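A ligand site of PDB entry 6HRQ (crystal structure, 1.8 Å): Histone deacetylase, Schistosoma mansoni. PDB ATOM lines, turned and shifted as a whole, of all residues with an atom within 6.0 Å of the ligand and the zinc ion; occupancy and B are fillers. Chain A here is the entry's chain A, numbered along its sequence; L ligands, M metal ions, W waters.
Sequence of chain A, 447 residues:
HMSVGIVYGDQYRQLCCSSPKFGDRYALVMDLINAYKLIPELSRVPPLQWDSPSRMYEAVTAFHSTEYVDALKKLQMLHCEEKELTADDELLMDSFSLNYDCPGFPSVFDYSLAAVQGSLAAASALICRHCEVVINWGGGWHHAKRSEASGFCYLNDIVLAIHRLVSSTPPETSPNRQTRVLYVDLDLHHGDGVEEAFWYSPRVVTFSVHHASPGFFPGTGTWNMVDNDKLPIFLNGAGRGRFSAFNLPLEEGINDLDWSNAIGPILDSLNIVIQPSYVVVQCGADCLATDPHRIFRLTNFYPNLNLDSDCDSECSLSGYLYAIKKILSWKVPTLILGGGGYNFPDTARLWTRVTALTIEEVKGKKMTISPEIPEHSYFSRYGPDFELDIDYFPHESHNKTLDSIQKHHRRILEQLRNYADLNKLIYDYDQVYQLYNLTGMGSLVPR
An oxygen (O2) of the ligand sits close to the side-chain hydroxyl of Tyr 342, 2.5 Å away. NE2 of His 143 is in hydrogen-bond range of N4 of the ligand. NE2 of His 142 sits close to O1 of the ligand, 2.8 Å away.
The side-chain carboxylate (OD1) of Asp 286 sits at hydrogen-bond distance from the backbone NH (N) of Leu 188, 3.0 Å away. The side-chain carboxylate (OD2) of Asp 187 is in hydrogen-bond range of the backbone NH (N) of Gly 340 (3.1 Å). The side-chain carboxylate (OD2) of Asp 187 sits at hydrogen-bond distance from the side-chain amide nitrogen (NE2) of Gln 282, 3.1 Å away. N of Tyr 342 sits at hydrogen-bond distance from OD2 of Asp 291 (2.9 Å). A ring nitrogen (NE2) of His 143 lies within hydrogen-bond range of a ring nitrogen (NE2) of His 142. N of His 143 lies within hydrogen-bond range of SG of Cys 153 (3.6 Å). A ring nitrogen (ND1) of His 293 lies within hydrogen-bond range of the side-chain carboxylate (OD1) of Asp 291. The backbone carbonyl oxygen (O) of Gly 151 lies within hydrogen-bond range of the side-chain sulfur (SG) of Cys 153 (3.7 Å).
The zinc ion is bound by the side-chain carboxylate (OD2) of Asp 286 (2.0 Å), the side-chain carboxylate (OD1) of Asp 187 (2.1 Å), a ring nitrogen (ND1) of His 189 (2.2 Å), an oxygen (O1) of the ligand (2.3 Å) and an oxygen (O2) of the ligand (2.3 Å).
NZ of Lys 21 touches C16 of the ligand, 3.2 Å away. Gly 151 touches the ligand. Phe 152 touches the ligand. CD2 of Phe 217 touches C11 of the ligand, at 3.6 Å. Pro 292 touches the ligand (O to C2, 3.6 Å). His 293 touches the ligand (N to C1, 3.8 Å). Gly 340 touches the ligand (CA to O2, 3.9 Å). Hydrophobic or aromatic side chains that line the ligand: His 142, His 143, Phe 152, His 189, Phe 217, Pro 292, His 293 and Tyr 342. Along chain A the residues within 4 Å of the ligand span positions 21 to 342. The nearest printed residue that does not touch the ligand is Asp 101 (4.8 Å).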
ATOM      1  N   LYS A  21       7.264   9.155  21.186  1.00  0.00           N
ATOM      2  CA  LYS A  21       5.934   9.042  20.602  1.00  0.00           C
ATOM      3  C   LYS A  21       5.916   8.140  19.362  1.00  0.00           C
ATOM      4  O   LYS A  21       4.964   7.379  19.154  1.00  0.00           O
ATOM      5  CB  LYS A  21       5.395  10.415  20.232  1.00  0.00           C
ATOM      6  CG  LYS A  21       3.993  10.378  19.692  1.00  0.00           C
ATOM      7  CD  LYS A  21       3.073   9.717  20.702  1.00  0.00           C
ATOM      8  CE  LYS A  21       1.742   9.302  20.096  1.00  0.00           C
ATOM      9  NZ  LYS A  21       0.853   8.731  21.140  1.00  0.00           N
ATOM     10  N   PHE A  22       6.941   8.233  18.508  1.00  0.00           N
ATOM     11  CA  PHE A  22       6.911   7.506  17.243  1.00  0.00           C
ATOM     12  C   PHE A  22       7.819   6.290  17.223  1.00  0.00           C
ATOM     13  O   PHE A  22       7.772   5.519  16.252  1.00  0.00           O
ATOM     14  CB  PHE A  22       7.239   8.470  16.088  1.00  0.00           C
ATOM     15  CG  PHE A  22       6.128   9.453  15.809  1.00  0.00           C
ATOM     16  CD1 PHE A  22       4.984   9.060  15.126  1.00  0.00           C
ATOM     17  CD2 PHE A  22       6.217  10.764  16.263  1.00  0.00           C
ATOM     18  CE1 PHE A  22       3.946   9.960  14.894  1.00  0.00           C
ATOM     19  CE2 PHE A  22       5.196  11.679  16.032  1.00  0.00           C
ATOM     20  CZ  PHE A  22       4.056  11.275  15.342  1.00  0.00           C
ATOM     21  N   ASP A 101       2.226  17.397  25.260  1.00  0.00           N
ATOM     22  CA  ASP A 101       2.473  16.510  24.136  1.00  0.00           C
ATOM     23  C   ASP A 101       3.779  16.796  23.422  1.00  0.00           C
ATOM     24  O   ASP A 101       4.142  16.039  22.509  1.00  0.00           O
ATOM     25  CB  ASP A 101       1.310  16.583  23.139  1.00  0.00           C
ATOM     26  CG  ASP A 101       0.070  15.909  23.651  1.00  0.00           C
ATOM     27  OD1 ASP A 101       0.209  14.924  24.405  1.00  0.00           O
ATOM     28  OD2 ASP A 101      -1.037  16.370  23.318  1.00  0.00           O
ATOM     29  N   HIS A 142       3.393  19.095  10.475  1.00  0.00           N
ATOM     30  CA  HIS A 142       2.700  20.291  10.017  1.00  0.00           C
ATOM     31  C   HIS A 142       2.180  21.205  11.122  1.00  0.00           C
ATOM     32  O   HIS A 142       1.703  22.301  10.812  1.00  0.00           O
ATOM     33  CB  HIS A 142       1.515  19.908   9.082  1.00  0.00           C
ATOM     34  CG  HIS A 142       0.546  18.929   9.664  1.00  0.00           C
ATOM     35  ND1 HIS A 142      -0.633  18.598   9.015  1.00  0.00           N
ATOM     36  CD2 HIS A 142       0.569  18.199  10.809  1.00  0.00           C
ATOM     37  CE1 HIS A 142      -1.291  17.705   9.743  1.00  0.00           C
ATOM     38  NE2 HIS A 142      -0.583  17.451  10.831  1.00  0.00           N
ATOM     39  N   HIS A 143       2.280  20.817  12.410  1.00  0.00           N
ATOM     40  CA  HIS A 143       1.657  21.622  13.465  1.00  0.00           C
ATOM     41  C   HIS A 143       2.568  22.661  14.106  1.00  0.00           C
ATOM     42  O   HIS A 143       2.065  23.553  14.799  1.00  0.00           O
ATOM     43  CB  HIS A 143       1.126  20.720  14.602  1.00  0.00           C
ATOM     44  CG  HIS A 143      -0.022  19.854  14.217  1.00  0.00           C
ATOM     45  ND1 HIS A 143      -1.170  20.337  13.625  1.00  0.00           N
ATOM     46  CD2 HIS A 143      -0.228  18.518  14.381  1.00  0.00           C
ATOM     47  CE1 HIS A 143      -2.018  19.343  13.424  1.00  0.00           C
ATOM     48  NE2 HIS A 143      -1.466  18.229  13.861  1.00  0.00           N
ATOM     49  N   GLY A 151       1.348  19.422  19.014  1.00  0.00           N
ATOM     50  CA  GLY A 151       0.926  18.145  18.425  1.00  0.00           C
ATOM     51  C   GLY A 151       2.044  17.199  18.029  1.00  0.00           C
ATOM     52  O   GLY A 151       1.986  16.579  16.961  1.00  0.00           O
ATOM     53  N   PHE A 152       3.057  17.052  18.894  1.00  0.00           N
ATOM     54  CA  PHE A 152       4.268  16.236  18.670  1.00  0.00           C
ATOM     55  C   PHE A 152       5.196  16.820  17.605  1.00  0.00           C
ATOM     56  O   PHE A 152       6.149  16.145  17.200  1.00  0.00           O
ATOM     57  CB  PHE A 152       3.977  14.784  18.261  1.00  0.00           C
ATOM     58  CG  PHE A 152       2.897  14.099  19.074  1.00  0.00           C
ATOM     59  CD1 PHE A 152       2.759  14.321  20.435  1.00  0.00           C
ATOM     60  CD2 PHE A 152       2.006  13.228  18.451  1.00  0.00           C
ATOM     61  CE1 PHE A 152       1.752  13.689  21.162  1.00  0.00           C
ATOM     62  CE2 PHE A 152       1.011  12.590  19.182  1.00  0.00           C
ATOM     63  CZ  PHE A 152       0.882  12.823  20.533  1.00  0.00           C
ATOM     64  N   CYS A 153       4.950  18.046  17.137  1.00  0.00           N
ATOM     65  CA  CYS A 153       5.783  18.709  16.138  1.00  0.00           C
ATOM     66  C   CYS A 153       6.579  19.826  16.806  1.00  0.00           C
ATOM     67  O   CYS A 153       6.001  20.696  17.459  1.00  0.00           O
ATOM     68  CB  CYS A 153       4.943  19.301  15.002  1.00  0.00           C
ATOM     69  SG  CYS A 153       3.836  18.111  14.184  1.00  0.00           S
ATOM     70  N   ASP A 187      -3.642  14.498   6.071  1.00  0.00           N
ATOM     71  CA  ASP A 187      -3.656  14.016   7.453  1.00  0.00           C
ATOM     72  C   ASP A 187      -5.073  14.090   8.060  1.00  0.00           C
ATOM     73  O   ASP A 187      -5.894  14.911   7.665  1.00  0.00           O
ATOM     74  CB  ASP A 187      -2.691  14.871   8.264  1.00  0.00           C
ATOM     75  CG  ASP A 187      -2.298  14.254   9.603  1.00  0.00           C
ATOM     76  OD1 ASP A 187      -3.073  14.396  10.584  1.00  0.00           O
ATOM     77  OD2 ASP A 187      -1.192  13.700   9.699  1.00  0.00           O
ATOM     78  N   LEU A 188      -5.346  13.223   9.052  1.00  0.00           N
ATOM     79  CA  LEU A 188      -6.595  13.321   9.807  1.00  0.00           C
ATOM     80  C   LEU A 188      -6.793  14.707  10.427  1.00  0.00           C
ATOM     81  O   LEU A 188      -7.937  15.174  10.541  1.00  0.00           O
ATOM     82  CB  LEU A 188      -6.638  12.274  10.924  1.00  0.00           C
ATOM     83  CG  LEU A 188      -7.913  12.234  11.786  1.00  0.00           C
ATOM     84  CD1 LEU A 188      -9.090  11.750  10.939  1.00  0.00           C
ATOM     85  CD2 LEU A 188      -7.720  11.309  12.977  1.00  0.00           C
ATOM     86  N   HIS A 189      -5.721  15.378  10.815  1.00  0.00           N
ATOM     87  CA  HIS A 189      -5.785  16.661  11.495  1.00  0.00           C
ATOM     88  C   HIS A 189      -5.589  17.841  10.528  1.00  0.00           C
ATOM     89  O   HIS A 189      -4.936  17.717   9.486  1.00  0.00           O
ATOM     90  CB  HIS A 189      -4.728  16.734  12.610  1.00  0.00           C
ATOM     91  CG  HIS A 189      -4.876  15.668  13.652  1.00  0.00           C
ATOM     92  ND1 HIS A 189      -4.229  14.462  13.575  1.00  0.00           N
ATOM     93  CD2 HIS A 189      -5.639  15.622  14.770  1.00  0.00           C
ATOM     94  CE1 HIS A 189      -4.571  13.712  14.618  1.00  0.00           C
ATOM     95  NE2 HIS A 189      -5.417  14.397  15.368  1.00  0.00           N
ATOM     96  N   HIS A 190      -6.165  18.989  10.892  1.00  0.00           N
ATOM     97  CA  HIS A 190      -5.954  20.216  10.145  1.00  0.00           C
ATOM     98  C   HIS A 190      -4.481  20.611  10.160  1.00  0.00           C
ATOM     99  O   HIS A 190      -3.842  20.640  11.217  1.00  0.00           O
ATOM    100  CB  HIS A 190      -6.811  21.348  10.734  1.00  0.00           C
ATOM    101  CG  HIS A 190      -6.556  22.696  10.115  1.00  0.00           C
ATOM    102  ND1 HIS A 190      -6.249  23.817  10.850  1.00  0.00           N
ATOM    103  CD2 HIS A 190      -6.598  23.095   8.821  1.00  0.00           C
ATOM    104  CE1 HIS A 190      -6.100  24.851  10.041  1.00  0.00           C
ATOM    105  NE2 HIS A 190      -6.322  24.443   8.801  1.00  0.00           N
ATOM    106  N   PHE A 217      -8.540  18.107  18.267  1.00  0.00           N
ATOM    107  CA  PHE A 217      -7.290  18.796  17.937  1.00  0.00           C
ATOM    108  C   PHE A 217      -7.149  19.077  16.437  1.00  0.00           C
ATOM    109  O   PHE A 217      -7.472  18.204  15.633  1.00  0.00           O
ATOM    110  CB  PHE A 217      -6.100  17.951  18.422  1.00  0.00           C
ATOM    111  CG  PHE A 217      -4.761  18.634  18.304  1.00  0.00           C
ATOM    112  CD1 PHE A 217      -4.267  19.395  19.352  1.00  0.00           C
ATOM    113  CD2 PHE A 217      -3.993  18.505  17.153  1.00  0.00           C
ATOM    114  CE1 PHE A 217      -3.041  20.027  19.265  1.00  0.00           C
ATOM    115  CE2 PHE A 217      -2.762  19.139  17.054  1.00  0.00           C
ATOM    116  CZ  PHE A 217      -2.283  19.898  18.095  1.00  0.00           C
ATOM    117  N   GLN A 282       1.347  16.228   2.144  1.00  0.00           N
ATOM    118  CA  GLN A 282       1.477  15.602   3.454  1.00  0.00           C
ATOM    119  C   GLN A 282       0.533  14.403   3.484  1.00  0.00           C
ATOM    120  O   GLN A 282      -0.664  14.540   3.212  1.00  0.00           O
ATOM    121  CB  GLN A 282       1.153  16.606   4.573  1.00  0.00           C
ATOM    122  CG  GLN A 282       1.699  16.267   5.969  1.00  0.00           C
ATOM    123  CD  GLN A 282       0.715  15.444   6.792  1.00  0.00           C
ATOM    124  OE1 GLN A 282      -0.196  14.821   6.244  1.00  0.00           O
ATOM    125  NE2 GLN A 282       0.902  15.428   8.116  1.00  0.00           N
ATOM    126  N   ASP A 286      -3.157   8.696   9.677  1.00  0.00           N
ATOM    127  CA  ASP A 286      -4.110   8.510  10.753  1.00  0.00           C
ATOM    128  C   ASP A 286      -5.572   8.551  10.301  1.00  0.00           C
ATOM    129  O   ASP A 286      -6.466   8.435  11.149  1.00  0.00           O
ATOM    130  CB  ASP A 286      -3.864   9.519  11.908  1.00  0.00           C
ATOM    131  CG  ASP A 286      -3.436  10.913  11.433  1.00  0.00           C
ATOM    132  OD1 ASP A 286      -3.461  11.208  10.223  1.00  0.00           O
ATOM    133  OD2 ASP A 286      -3.095  11.728  12.320  1.00  0.00           O
ATOM    134  N   ASP A 291      -6.313   2.939  12.326  1.00  0.00           N
ATOM    135  CA  ASP A 291      -5.611   3.827  13.260  1.00  0.00           C
ATOM    136  C   ASP A 291      -6.358   3.854  14.588  1.00  0.00           C
ATOM    137  O   ASP A 291      -7.592   3.812  14.598  1.00  0.00           O
ATOM    138  CB  ASP A 291      -5.493   5.236  12.680  1.00  0.00           C
ATOM    139  CG  ASP A 291      -4.521   6.119  13.467  1.00  0.00           C
ATOM    140  OD1 ASP A 291      -4.958   6.719  14.473  1.00  0.00           O
ATOM    141  OD2 ASP A 291      -3.331   6.209  13.093  1.00  0.00           O
ATOM    142  N   PRO A 292      -5.659   3.898  15.725  1.00  0.00           N
ATOM    143  CA  PRO A 292      -6.367   3.930  17.016  1.00  0.00           C
ATOM    144  C   PRO A 292      -7.308   5.112  17.187  1.00  0.00           C
ATOM    145  O   PRO A 292      -8.206   5.053  18.043  1.00  0.00           O
ATOM    146  CB  PRO A 292      -5.239   3.971  18.062  1.00  0.00           C
ATOM    147  CG  PRO A 292      -3.967   3.768  17.316  1.00  0.00           C
ATOM    148  CD  PRO A 292      -4.196   3.924  15.865  1.00  0.00           C
ATOM    149  N   HIS A 293      -7.133   6.202  16.420  1.00  0.00           N
ATOM    150  CA  HIS A 293      -8.130   7.272  16.414  1.00  0.00           C
ATOM    151  C   HIS A 293      -9.511   6.742  16.055  1.00  0.00           C
ATOM    152  O   HIS A 293     -10.528   7.178  16.614  1.00  0.00           O
ATOM    153  CB  HIS A 293      -7.734   8.387  15.440  1.00  0.00           C
ATOM    154  CG  HIS A 293      -6.666   9.292  15.961  1.00  0.00           C
ATOM    155  ND1 HIS A 293      -5.326   9.112  15.676  1.00  0.00           N
ATOM    156  CD2 HIS A 293      -6.739  10.412  16.729  1.00  0.00           C
ATOM    157  CE1 HIS A 293      -4.626  10.076  16.243  1.00  0.00           C
ATOM    158  NE2 HIS A 293      -5.449  10.877  16.888  1.00  0.00           N
ATOM    159  N   ARG A 294      -9.575   5.819  15.085  1.00  0.00           N
ATOM    160  CA  ARG A 294     -10.842   5.245  14.634  1.00  0.00           C
ATOM    161  C   ARG A 294     -11.863   6.338  14.314  1.00  0.00           C
ATOM    162  O   ARG A 294     -12.993   6.319  14.807  1.00  0.00           O
ATOM    163  CB  ARG A 294     -11.383   4.275  15.680  1.00  0.00           C
ATOM    164  CG  ARG A 294     -10.421   3.162  16.073  1.00  0.00           C
ATOM    165  CD  ARG A 294     -10.278   2.136  14.955  1.00  0.00           C
ATOM    166  NE  ARG A 294      -9.566   0.941  15.383  1.00  0.00           N
ATOM    167  CZ  ARG A 294      -9.641  -0.242  14.762  1.00  0.00           C
ATOM    168  NH1 ARG A 294     -10.402  -0.380  13.685  1.00  0.00           N
ATOM    169  NH2 ARG A 294      -8.955  -1.278  15.233  1.00  0.00           N
ATOM    170  N   GLY A 339       3.871  12.032   8.206  1.00  0.00           N
ATOM    171  CA  GLY A 339       3.073  12.748   9.178  1.00  0.00           C
ATOM    172  C   GLY A 339       2.519  11.824  10.241  1.00  0.00           C
ATOM    173  O   GLY A 339       3.225  10.942  10.736  1.00  0.00           O
ATOM    174  N   GLY A 340       1.250  11.993  10.600  1.00  0.00           N
ATOM    175  CA  GLY A 340       0.625  11.125  11.589  1.00  0.00           C
ATOM    176  C   GLY A 340       0.527   9.672  11.126  1.00  0.00           C
ATOM    177  O   GLY A 340       0.789   9.300   9.984  1.00  0.00           O
ATOM    178  N   GLY A 341       0.134   8.826  12.080  1.00  0.00           N
ATOM    179  CA  GLY A 341      -0.032   7.397  11.847  1.00  0.00           C
ATOM    180  C   GLY A 341       0.444   6.613  13.056  1.00  0.00           C
ATOM    181  O   GLY A 341       1.655   6.433  13.265  1.00  0.00           O
ATOM    182  N   TYR A 342      -0.491   6.114  13.870  1.00  0.00           N
ATOM    183  CA  TYR A 342      -0.156   5.556  15.180  1.00  0.00           C
ATOM    184  C   TYR A 342      -0.376   4.051  15.252  1.00  0.00           C
ATOM    185  O   TYR A 342      -0.136   3.448  16.302  1.00  0.00           O
ATOM    186  CB  TYR A 342      -0.932   6.334  16.247  1.00  0.00           C
ATOM    187  CG  TYR A 342      -0.599   7.799  16.037  1.00  0.00           C
ATOM    188  CD1 TYR A 342       0.595   8.324  16.529  1.00  0.00           C
ATOM    189  CD2 TYR A 342      -1.403   8.619  15.241  1.00  0.00           C
ATOM    190  CE1 TYR A 342       0.958   9.659  16.289  1.00  0.00           C
ATOM    191  CE2 TYR A 342      -1.035   9.956  14.988  1.00  0.00           C
ATOM    192  CZ  TYR A 342       0.147  10.451  15.516  1.00  0.00           C
ATOM    193  OH  TYR A 342       0.514  11.769  15.290  1.00  0.00           O
HETATM  194  C1  LIG L   1      -5.590   7.927  19.435  1.00  0.00           C
HETATM  195  C2  LIG L   1      -6.813   7.652  20.037  1.00  0.00           C
HETATM  196  C3  LIG L   1      -6.899   6.658  20.983  1.00  0.00           C
HETATM  197  C4  LIG L   1      -4.562   6.205  20.754  1.00  0.00           C
HETATM  198  C5  LIG L   1      -2.409  12.009  19.165  1.00  0.00           C
HETATM  199  C6  LIG L   1      -1.736  15.596  16.979  1.00  0.00           C
HETATM  200  C7  LIG L   1      -1.616  14.370  16.329  1.00  0.00           C
HETATM  201  C8  LIG L   1      -1.818  13.200  17.065  1.00  0.00           C
HETATM  202  C9  LIG L   1      -2.161  13.255  18.412  1.00  0.00           C
HETATM  203  C10 LIG L   1      -2.278  14.501  19.035  1.00  0.00           C
HETATM  204  C11 LIG L   1      -2.058  15.656  18.320  1.00  0.00           C
HETATM  205  C12 LIG L   1      -1.365  14.318  14.854  1.00  0.00           C
HETATM  206  C13 LIG L   1      -4.465   7.203  19.781  1.00  0.00           C
HETATM  207  C14 LIG L   1      -5.780   5.931  21.343  1.00  0.00           C
HETATM  208  N1  LIG L   1      -2.436  10.015  19.971  1.00  0.00           N
HETATM  209  N2  LIG L   1      -3.342  10.724  20.661  1.00  0.00           N
HETATM  210  N3  LIG L   1      -3.332  11.946  20.171  1.00  0.00           N
HETATM  211  C15 LIG L   1      -1.841  10.773  19.045  1.00  0.00           C
HETATM  212  N4  LIG L   1      -1.380  15.485  14.215  1.00  0.00           N
HETATM  213  O1  LIG L   1      -1.266  15.536  12.824  1.00  0.00           O
HETATM  214  O2  LIG L   1      -1.197  13.238  14.283  1.00  0.00           O
HETATM  215  S1  LIG L   1      -2.916   7.527  19.001  1.00  0.00           S
HETATM  216  C16 LIG L   1      -2.176   8.616  20.249  1.00  0.00           C
HETATM  217 ZN    ZN M   1      -2.532  13.671  12.465  1.00  0.00          ZN
HETATM  218  O   HOH W   1       1.707  14.881  12.057  1.00  0.00           O
HETATM  219  O   HOH W   2      -5.147  13.684  20.930  1.00  0.00           O
